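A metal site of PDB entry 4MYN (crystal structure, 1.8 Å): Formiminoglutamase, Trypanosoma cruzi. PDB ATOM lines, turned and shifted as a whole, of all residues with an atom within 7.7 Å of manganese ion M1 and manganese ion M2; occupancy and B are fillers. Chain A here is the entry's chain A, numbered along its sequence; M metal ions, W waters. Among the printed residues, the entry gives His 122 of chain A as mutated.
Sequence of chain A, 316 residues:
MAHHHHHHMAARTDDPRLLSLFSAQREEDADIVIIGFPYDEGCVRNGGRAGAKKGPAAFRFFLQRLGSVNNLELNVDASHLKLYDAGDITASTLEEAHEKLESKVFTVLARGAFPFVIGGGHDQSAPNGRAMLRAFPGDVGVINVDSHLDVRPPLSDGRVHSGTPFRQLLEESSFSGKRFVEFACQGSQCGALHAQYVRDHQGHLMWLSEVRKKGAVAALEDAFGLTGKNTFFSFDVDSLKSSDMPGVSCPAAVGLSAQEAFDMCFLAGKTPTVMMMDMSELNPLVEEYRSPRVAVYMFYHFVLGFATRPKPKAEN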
ATOM      1  N   ASN A  46       1.785   5.060  -3.884  1.00  0.00           N
ATOM      2  CA  ASN A  46       2.901   4.592  -4.718  1.00  0.00           C
ATOM      3  C   ASN A  46       2.851   5.273  -6.091  1.00  0.00           C
ATOM      4  O   ASN A  46       3.434   4.789  -7.064  1.00  0.00           O
ATOM      5  CB  ASN A  46       2.825   3.068  -4.863  1.00  0.00           C
ATOM      6  CG  ASN A  46       4.061   2.469  -5.524  1.00  0.00           C
ATOM      7  OD1 ASN A  46       5.181   2.983  -5.376  1.00  0.00           O
ATOM      8  ND2 ASN A  46       3.867   1.368  -6.252  1.00  0.00           N
ATOM      9  N   GLY A 121      -5.341  -2.810  -3.997  1.00  0.00           N
ATOM     10  CA  GLY A 121      -3.913  -2.603  -4.200  1.00  0.00           C
ATOM     11  C   GLY A 121      -3.061  -3.737  -3.662  1.00  0.00           C
ATOM     12  O   GLY A 121      -3.481  -4.458  -2.761  1.00  0.00           O
ATOM     13  N   HIS A 122      -1.848  -3.862  -4.182  1.00  0.00           N
ATOM     14  CA  HIS A 122      -0.960  -4.954  -3.807  1.00  0.00           C
ATOM     15  C   HIS A 122      -0.432  -4.858  -2.378  1.00  0.00           C
ATOM     16  O   HIS A 122       0.161  -5.810  -1.873  1.00  0.00           O
ATOM     17  CB  HIS A 122       0.225  -5.041  -4.775  1.00  0.00           C
ATOM     18  CG  HIS A 122       0.780  -6.424  -4.936  1.00  0.00           C
ATOM     19  ND1 HIS A 122       1.747  -6.742  -5.857  1.00  0.00           N
ATOM     20  CD2 HIS A 122       0.484  -7.581  -4.279  1.00  0.00           C
ATOM     21  CE1 HIS A 122       2.040  -8.028  -5.768  1.00  0.00           C
ATOM     22  NE2 HIS A 122       1.275  -8.562  -4.824  1.00  0.00           N
ATOM     23  N   ASP A 123      -0.640  -3.713  -1.730  1.00  0.00           N
ATOM     24  CA  ASP A 123      -0.270  -3.594  -0.318  1.00  0.00           C
ATOM     25  C   ASP A 123      -0.908  -4.683   0.567  1.00  0.00           C
ATOM     26  O   ASP A 123      -0.390  -4.987   1.651  1.00  0.00           O
ATOM     27  CB  ASP A 123      -0.564  -2.197   0.240  1.00  0.00           C
ATOM     28  CG  ASP A 123      -1.941  -1.680  -0.157  1.00  0.00           C
ATOM     29  OD1 ASP A 123      -2.133  -1.364  -1.373  1.00  0.00           O
ATOM     30  OD2 ASP A 123      -2.813  -1.565   0.735  1.00  0.00           O
ATOM     31  N   SER A 125      -0.698  -7.672   0.273  1.00  0.00           N
ATOM     32  CA  SER A 125       0.170  -8.841   0.378  1.00  0.00           C
ATOM     33  C   SER A 125       1.010  -8.855   1.653  1.00  0.00           C
ATOM     34  O   SER A 125       1.468  -9.914   2.069  1.00  0.00           O
ATOM     35  CB  SER A 125       1.043  -8.973  -0.863  1.00  0.00           C
ATOM     36  OG  SER A 125       0.213  -9.250  -1.970  1.00  0.00           O
ATOM     37  N   ASN A 144       5.976 -13.748  -5.831  1.00  0.00           N
ATOM     38  CA  ASN A 144       5.302 -12.549  -6.285  1.00  0.00           C
ATOM     39  C   ASN A 144       5.302 -12.524  -7.811  1.00  0.00           C
ATOM     40  O   ASN A 144       6.342 -12.293  -8.439  1.00  0.00           O
ATOM     41  CB  ASN A 144       5.986 -11.297  -5.745  1.00  0.00           C
ATOM     42  CG  ASN A 144       5.342 -10.017  -6.234  1.00  0.00           C
ATOM     43  OD1 ASN A 144       4.133  -9.966  -6.452  1.00  0.00           O
ATOM     44  ND2 ASN A 144       6.142  -8.992  -6.447  1.00  0.00           N
ATOM     45  N   VAL A 145       4.128 -12.765  -8.409  1.00  0.00           N
ATOM     46  CA  VAL A 145       4.004 -12.686  -9.862  1.00  0.00           C
ATOM     47  C   VAL A 145       3.656 -11.234 -10.172  1.00  0.00           C
ATOM     48  O   VAL A 145       2.545 -10.772  -9.875  1.00  0.00           O
ATOM     49  CB  VAL A 145       2.905 -13.607 -10.433  1.00  0.00           C
ATOM     50  CG1 VAL A 145       2.891 -13.523 -11.980  1.00  0.00           C
ATOM     51  CG2 VAL A 145       3.130 -15.062  -9.967  1.00  0.00           C
ATOM     52  N   ASP A 146       4.621 -10.534 -10.745  1.00  0.00           N
ATOM     53  CA  ASP A 146       4.542  -9.084 -10.836  1.00  0.00           C
ATOM     54  C   ASP A 146       5.554  -8.576 -11.847  1.00  0.00           C
ATOM     55  O   ASP A 146       6.701  -9.048 -11.884  1.00  0.00           O
ATOM     56  CB  ASP A 146       4.873  -8.531  -9.436  1.00  0.00           C
ATOM     57  CG  ASP A 146       4.415  -7.105  -9.248  1.00  0.00           C
ATOM     58  OD1 ASP A 146       4.297  -6.364 -10.239  1.00  0.00           O
ATOM     59  OD2 ASP A 146       4.193  -6.741  -8.070  1.00  0.00           O
ATOM     60  N   SER A 147       5.179  -7.610 -12.672  1.00  0.00           N
ATOM     61  CA  SER A 147       6.189  -6.942 -13.503  1.00  0.00           C
ATOM     62  C   SER A 147       7.177  -6.139 -12.637  1.00  0.00           C
ATOM     63  O   SER A 147       8.294  -5.857 -13.074  1.00  0.00           O
ATOM     64  CB  SER A 147       5.542  -6.051 -14.561  1.00  0.00           C
ATOM     65  OG  SER A 147       4.641  -5.141 -13.964  1.00  0.00           O
ATOM     66  N   HIS A 148       6.760  -5.777 -11.433  1.00  0.00           N
ATOM     67  CA  HIS A 148       7.567  -4.957 -10.521  1.00  0.00           C
ATOM     68  C   HIS A 148       8.048  -5.759  -9.298  1.00  0.00           C
ATOM     69  O   HIS A 148       7.437  -6.735  -8.953  1.00  0.00           O
ATOM     70  CB  HIS A 148       6.752  -3.763 -10.034  1.00  0.00           C
ATOM     71  CG  HIS A 148       5.953  -3.121 -11.125  1.00  0.00           C
ATOM     72  ND1 HIS A 148       4.607  -3.397 -11.329  1.00  0.00           N
ATOM     73  CD2 HIS A 148       6.312  -2.229 -12.078  1.00  0.00           C
ATOM     74  CE1 HIS A 148       4.182  -2.688 -12.361  1.00  0.00           C
ATOM     75  NE2 HIS A 148       5.189  -1.980 -12.840  1.00  0.00           N
ATOM     76  N   LEU A 149       9.117  -5.308  -8.631  1.00  0.00           N
ATOM     77  CA  LEU A 149       9.644  -6.068  -7.487  1.00  0.00           C
ATOM     78  C   LEU A 149       8.905  -5.774  -6.172  1.00  0.00           C
ATOM     79  O   LEU A 149       8.791  -6.654  -5.290  1.00  0.00           O
ATOM     80  CB  LEU A 149      11.147  -5.798  -7.294  1.00  0.00           C
ATOM     81  CG  LEU A 149      12.120  -6.265  -8.375  1.00  0.00           C
ATOM     82  CD1 LEU A 149      13.532  -6.095  -7.839  1.00  0.00           C
ATOM     83  CD2 LEU A 149      11.860  -7.710  -8.736  1.00  0.00           C
ATOM     84  N   ASP A 150       8.411  -4.554  -6.045  1.00  0.00           N
ATOM     85  CA  ASP A 150       7.593  -4.165  -4.895  1.00  0.00           C
ATOM     86  C   ASP A 150       8.355  -4.313  -3.579  1.00  0.00           C
ATOM     87  O   ASP A 150       7.810  -4.817  -2.590  1.00  0.00           O
ATOM     88  CB  ASP A 150       6.300  -4.976  -4.844  1.00  0.00           C
ATOM     89  CG  ASP A 150       5.279  -4.486  -5.852  1.00  0.00           C
ATOM     90  OD1 ASP A 150       5.679  -3.823  -6.841  1.00  0.00           O
ATOM     91  OD2 ASP A 150       4.076  -4.755  -5.636  1.00  0.00           O
ATOM     92  N   SER A 162       1.422   0.303  -2.249  1.00  0.00           N
ATOM     93  CA  SER A 162       1.357  -0.812  -3.194  1.00  0.00           C
ATOM     94  C   SER A 162       2.738  -1.309  -3.658  1.00  0.00           C
ATOM     95  O   SER A 162       2.836  -2.324  -4.345  1.00  0.00           O
ATOM     96  CB  SER A 162       0.436  -0.481  -4.396  1.00  0.00           C
ATOM     97  OG  SER A 162       0.957   0.564  -5.203  1.00  0.00           O
ATOM     98  N   GLY A 163       3.787  -0.598  -3.276  1.00  0.00           N
ATOM     99  CA  GLY A 163       5.133  -0.965  -3.700  1.00  0.00           C
ATOM    100  C   GLY A 163       6.051  -1.456  -2.591  1.00  0.00           C
ATOM    101  O   GLY A 163       7.219  -1.743  -2.848  1.00  0.00           O
ATOM    102  N   THR A 164       5.529  -1.563  -1.370  1.00  0.00           N
ATOM    103  CA  THR A 164       6.354  -2.003  -0.237  1.00  0.00           C
ATOM    104  C   THR A 164       6.111  -3.415   0.321  1.00  0.00           C
ATOM    105  O   THR A 164       6.879  -3.842   1.170  1.00  0.00           O
ATOM    106  CB  THR A 164       6.233  -1.035   0.943  1.00  0.00           C
ATOM    107  OG1 THR A 164       4.915  -1.126   1.489  1.00  0.00           O
ATOM    108  CG2 THR A 164       6.501   0.397   0.490  1.00  0.00           C
ATOM    109  N   PRO A 165       5.078  -4.129  -0.158  1.00  0.00           N
ATOM    110  CA  PRO A 165       4.658  -5.317   0.608  1.00  0.00           C
ATOM    111  C   PRO A 165       5.739  -6.373   0.809  1.00  0.00           C
ATOM    112  O   PRO A 165       5.736  -7.072   1.829  1.00  0.00           O
ATOM    113  CB  PRO A 165       3.531  -5.933  -0.250  1.00  0.00           C
ATOM    114  CG  PRO A 165       3.277  -4.973  -1.354  1.00  0.00           C
ATOM    115  CD  PRO A 165       4.426  -4.051  -1.474  1.00  0.00           C
ATOM    116  N   PHE A 166       6.651  -6.505  -0.151  1.00  0.00           N
ATOM    117  CA  PHE A 166       7.660  -7.567  -0.044  1.00  0.00           C
ATOM    118  C   PHE A 166       8.943  -7.090   0.610  1.00  0.00           C
ATOM    119  O   PHE A 166       9.808  -7.885   0.958  1.00  0.00           O
ATOM    120  CB  PHE A 166       7.863  -8.265  -1.385  1.00  0.00           C
ATOM    121  CG  PHE A 166       6.599  -8.879  -1.895  1.00  0.00           C
ATOM    122  CD1 PHE A 166       6.145 -10.081  -1.391  1.00  0.00           C
ATOM    123  CD2 PHE A 166       5.800  -8.181  -2.794  1.00  0.00           C
ATOM    124  CE1 PHE A 166       4.940 -10.617  -1.820  1.00  0.00           C
ATOM    125  CE2 PHE A 166       4.600  -8.712  -3.230  1.00  0.00           C
ATOM    126  CZ  PHE A 166       4.172  -9.928  -2.747  1.00  0.00           C
ATOM    127  N   GLU A 182      10.588 -13.601  -7.201  1.00  0.00           N
ATOM    128  CA  GLU A 182       9.967 -12.532  -7.959  1.00  0.00           C
ATOM    129  C   GLU A 182       9.805 -13.082  -9.371  1.00  0.00           C
ATOM    130  O   GLU A 182      10.792 -13.298 -10.070  1.00  0.00           O
ATOM    131  CB  GLU A 182      10.843 -11.294  -7.967  1.00  0.00           C
ATOM    132  CG  GLU A 182      11.071 -10.636  -6.580  1.00  0.00           C
ATOM    133  CD  GLU A 182      10.048  -9.551  -6.248  1.00  0.00           C
ATOM    134  OE1 GLU A 182       8.897  -9.607  -6.740  1.00  0.00           O
ATOM    135  OE2 GLU A 182      10.406  -8.634  -5.460  1.00  0.00           O
ATOM    136  N   GLN A 189      11.566  -2.033 -15.792  1.00  0.00           N
ATOM    137  CA  GLN A 189      10.707  -1.454 -14.762  1.00  0.00           C
ATOM    138  C   GLN A 189      11.238  -1.733 -13.366  1.00  0.00           C
ATOM    139  O   GLN A 189      10.590  -1.368 -12.376  1.00  0.00           O
ATOM    140  CB  GLN A 189       9.293  -2.063 -14.813  1.00  0.00           C
ATOM    141  CG  GLN A 189       8.576  -2.031 -16.142  1.00  0.00           C
ATOM    142  CD  GLN A 189       7.074  -2.022 -15.955  1.00  0.00           C
ATOM    143  OE1 GLN A 189       6.517  -1.115 -15.321  1.00  0.00           O
ATOM    144  NE2 GLN A 189       6.381  -3.036 -16.502  1.00  0.00           N
ATOM    145  N   SER A 234       1.075 -15.010  -4.846  1.00  0.00           N
ATOM    146  CA  SER A 234       0.637 -13.616  -4.889  1.00  0.00           C
ATOM    147  C   SER A 234       0.709 -13.108  -6.324  1.00  0.00           C
ATOM    148  O   SER A 234       1.791 -13.047  -6.910  1.00  0.00           O
ATOM    149  CB  SER A 234       1.510 -12.743  -3.986  1.00  0.00           C
ATOM    150  OG  SER A 234       1.033 -11.406  -3.918  1.00  0.00           O
ATOM    151  N   PHE A 235      -0.438 -12.736  -6.875  1.00  0.00           N
ATOM    152  CA  PHE A 235      -0.511 -12.408  -8.295  1.00  0.00           C
ATOM    153  C   PHE A 235      -0.905 -10.945  -8.479  1.00  0.00           C
ATOM    154  O   PHE A 235      -1.996 -10.533  -8.125  1.00  0.00           O
ATOM    155  CB  PHE A 235      -1.546 -13.327  -8.987  1.00  0.00           C
ATOM    156  CG  PHE A 235      -1.197 -13.669 -10.436  1.00  0.00           C
ATOM    157  CD1 PHE A 235      -0.895 -12.665 -11.346  1.00  0.00           C
ATOM    158  CD2 PHE A 235      -1.194 -14.987 -10.862  1.00  0.00           C
ATOM    159  CE1 PHE A 235      -0.597 -12.982 -12.688  1.00  0.00           C
ATOM    160  CE2 PHE A 235      -0.896 -15.305 -12.204  1.00  0.00           C
ATOM    161  CZ  PHE A 235      -0.587 -14.296 -13.107  1.00  0.00           C
ATOM    162  N   ASP A 236       0.008 -10.170  -9.056  1.00  0.00           N
ATOM    163  CA  ASP A 236      -0.287  -8.786  -9.448  1.00  0.00           C
ATOM    164  C   ASP A 236      -0.639  -8.837 -10.923  1.00  0.00           C
ATOM    165  O   ASP A 236       0.200  -9.192 -11.728  1.00  0.00           O
ATOM    166  CB  ASP A 236       0.952  -7.952  -9.290  1.00  0.00           C
ATOM    167  CG  ASP A 236       0.720  -6.486  -9.609  1.00  0.00           C
ATOM    168  OD1 ASP A 236      -0.271  -6.134 -10.273  1.00  0.00           O
ATOM    169  OD2 ASP A 236       1.544  -5.678  -9.179  1.00  0.00           O
ATOM    170  N   VAL A 237      -1.884  -8.488 -11.268  1.00  0.00           N
ATOM    171  CA  VAL A 237      -2.349  -8.676 -12.645  1.00  0.00           C
ATOM    172  C   VAL A 237      -1.675  -7.722 -13.650  1.00  0.00           C
ATOM    173  O   VAL A 237      -1.833  -7.880 -14.870  1.00  0.00           O
ATOM    174  CB  VAL A 237      -3.907  -8.642 -12.785  1.00  0.00           C
ATOM    175  CG1 VAL A 237      -4.538  -9.855 -12.108  1.00  0.00           C
ATOM    176  CG2 VAL A 237      -4.482  -7.328 -12.300  1.00  0.00           C
ATOM    177  N   ASP A 238      -0.904  -6.754 -13.145  1.00  0.00           N
ATOM    178  CA  ASP A 238      -0.102  -5.931 -14.050  1.00  0.00           C
ATOM    179  C   ASP A 238       1.161  -6.651 -14.553  1.00  0.00           C
ATOM    180  O   ASP A 238       1.984  -6.057 -15.243  1.00  0.00           O
ATOM    181  CB  ASP A 238       0.213  -4.538 -13.459  1.00  0.00           C
ATOM    182  CG  ASP A 238       1.268  -4.564 -12.352  1.00  0.00           C
ATOM    183  OD1 ASP A 238       2.108  -5.490 -12.286  1.00  0.00           O
ATOM    184  OD2 ASP A 238       1.270  -3.589 -11.558  1.00  0.00           O
ATOM    185  N   SER A 239       1.275  -7.948 -14.239  1.00  0.00           N
ATOM    186  CA  SER A 239       2.296  -8.803 -14.841  1.00  0.00           C
ATOM    187  C   SER A 239       1.825  -9.279 -16.213  1.00  0.00           C
ATOM    188  O   SER A 239       2.633  -9.764 -17.000  1.00  0.00           O
ATOM    189  CB  SER A 239       2.561 -10.045 -13.967  1.00  0.00           C
ATOM    190  OG  SER A 239       1.376 -10.830 -13.842  1.00  0.00           O
ATOM    191  N   CYS A 250      -0.940   0.184 -13.452  1.00  0.00           N
ATOM    192  CA  CYS A 250       0.296   0.318 -14.223  1.00  0.00           C
ATOM    193  C   CYS A 250       0.283  -0.695 -15.373  1.00  0.00           C
ATOM    194  O   CYS A 250       0.873  -1.763 -15.246  1.00  0.00           O
ATOM    195  CB  CYS A 250       1.546   0.075 -13.349  1.00  0.00           C
ATOM    196  SG  CYS A 250       3.178   0.398 -14.178  1.00  0.00           S
ATOM    197  N   SER A 280      -4.032  -8.780  -7.034  1.00  0.00           N
ATOM    198  CA  SER A 280      -4.016  -7.343  -6.768  1.00  0.00           C
ATOM    199  C   SER A 280      -3.935  -6.515  -8.068  1.00  0.00           C
ATOM    200  O   SER A 280      -3.513  -7.016  -9.111  1.00  0.00           O
ATOM    201  CB  SER A 280      -2.825  -6.982  -5.873  1.00  0.00           C
ATOM    202  OG  SER A 280      -2.870  -7.710  -4.659  1.00  0.00           O
ATOM    203  N   GLU A 281      -4.362  -5.267  -7.952  1.00  0.00           N
ATOM    204  CA  GLU A 281      -4.171  -4.220  -8.959  1.00  0.00           C
ATOM    205  C   GLU A 281      -5.228  -4.146 -10.061  1.00  0.00           C
ATOM    206  O   GLU A 281      -5.150  -3.303 -10.961  1.00  0.00           O
ATOM    207  CB  GLU A 281      -2.740  -4.217  -9.528  1.00  0.00           C
ATOM    208  CG  GLU A 281      -1.666  -3.995  -8.433  1.00  0.00           C
ATOM    209  CD  GLU A 281      -1.732  -2.609  -7.800  1.00  0.00           C
ATOM    210  OE1 GLU A 281      -1.958  -1.635  -8.553  1.00  0.00           O
ATOM    211  OE2 GLU A 281      -1.517  -2.486  -6.573  1.00  0.00           O
HETATM  212 MN    MN M   1       3.054  -4.603 -10.368  1.00  0.00          MN
HETATM  213 MN    MN M   2       2.672  -5.322  -7.301  1.00  0.00          MN
HETATM  214  O   HOH W   1       1.660  -3.241  -6.863  1.00  0.00           O
HETATM  215  O   HOH W   2       3.363  -3.499  -8.503  1.00  0.00           O
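A ring nitrogen (NE2) of His 122 lies within hydrogen-bond range of the side-chain hydroxyl (OG) of Ser 234 (3.0 Å).
OE1 of Gln 189 sits at hydrogen-bond distance from NE2 of His 148, at 2.9 Å.
The backbone carbonyl oxygen of Asp 150 lies within hydrogen-bond range of the backbone NH of Phe 166 (3.2 Å).
The side-chain hydroxyl (OG) of Ser 125 lies close to a ring nitrogen (NE2) of His 122 (3.1 Å).
N of His 122 is in hydrogen-bond range of OE2 of Glu 281 (2.8 Å).
The backbone NH of Asp 236 lies within hydrogen-bond range of the backbone carbonyl oxygen of Val 145.
A ring nitrogen (NE2) of His 148 is in hydrogen-bond range of the side-chain sulfur of Cys 250 (3.4 Å).
A ring nitrogen (NE2) of His 148 sits close to the side-chain hydroxyl (OG) of Ser 147 (3.4 Å).
Ser 147 touches manganese ion M1.
Of the 28 residues printed, 5 come within 4 Å of manganese ion M1.
Along chain A the residues within 4 Å of manganese ion M1 span positions 146 to 238.
Four residues have an atom within 4 Å of manganese ion M2: His 122, Asp 146, Asp 150 and Asp 236.
Manganese ion M1 is bound by OD1 of Asp 146, water W2, ND1 of His 148, OD2 of Asp 236, OD1 of Asp 238 and OD2 of Asp 238.
Manganese ion M2 is bound by OD2 of Asp 146, OD2 of Asp 236, ND1 of His 122, OD2 of Asp 150, water W2 and water W1.
Manganese ion M2 has six donor atoms within binding distance.
Water W1 bridges the backbone carbonyl oxygen (O) of Ser 162 (2.9 Å) and the side-chain carboxylate (OE2) of Glu 281 (3.3 Å).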
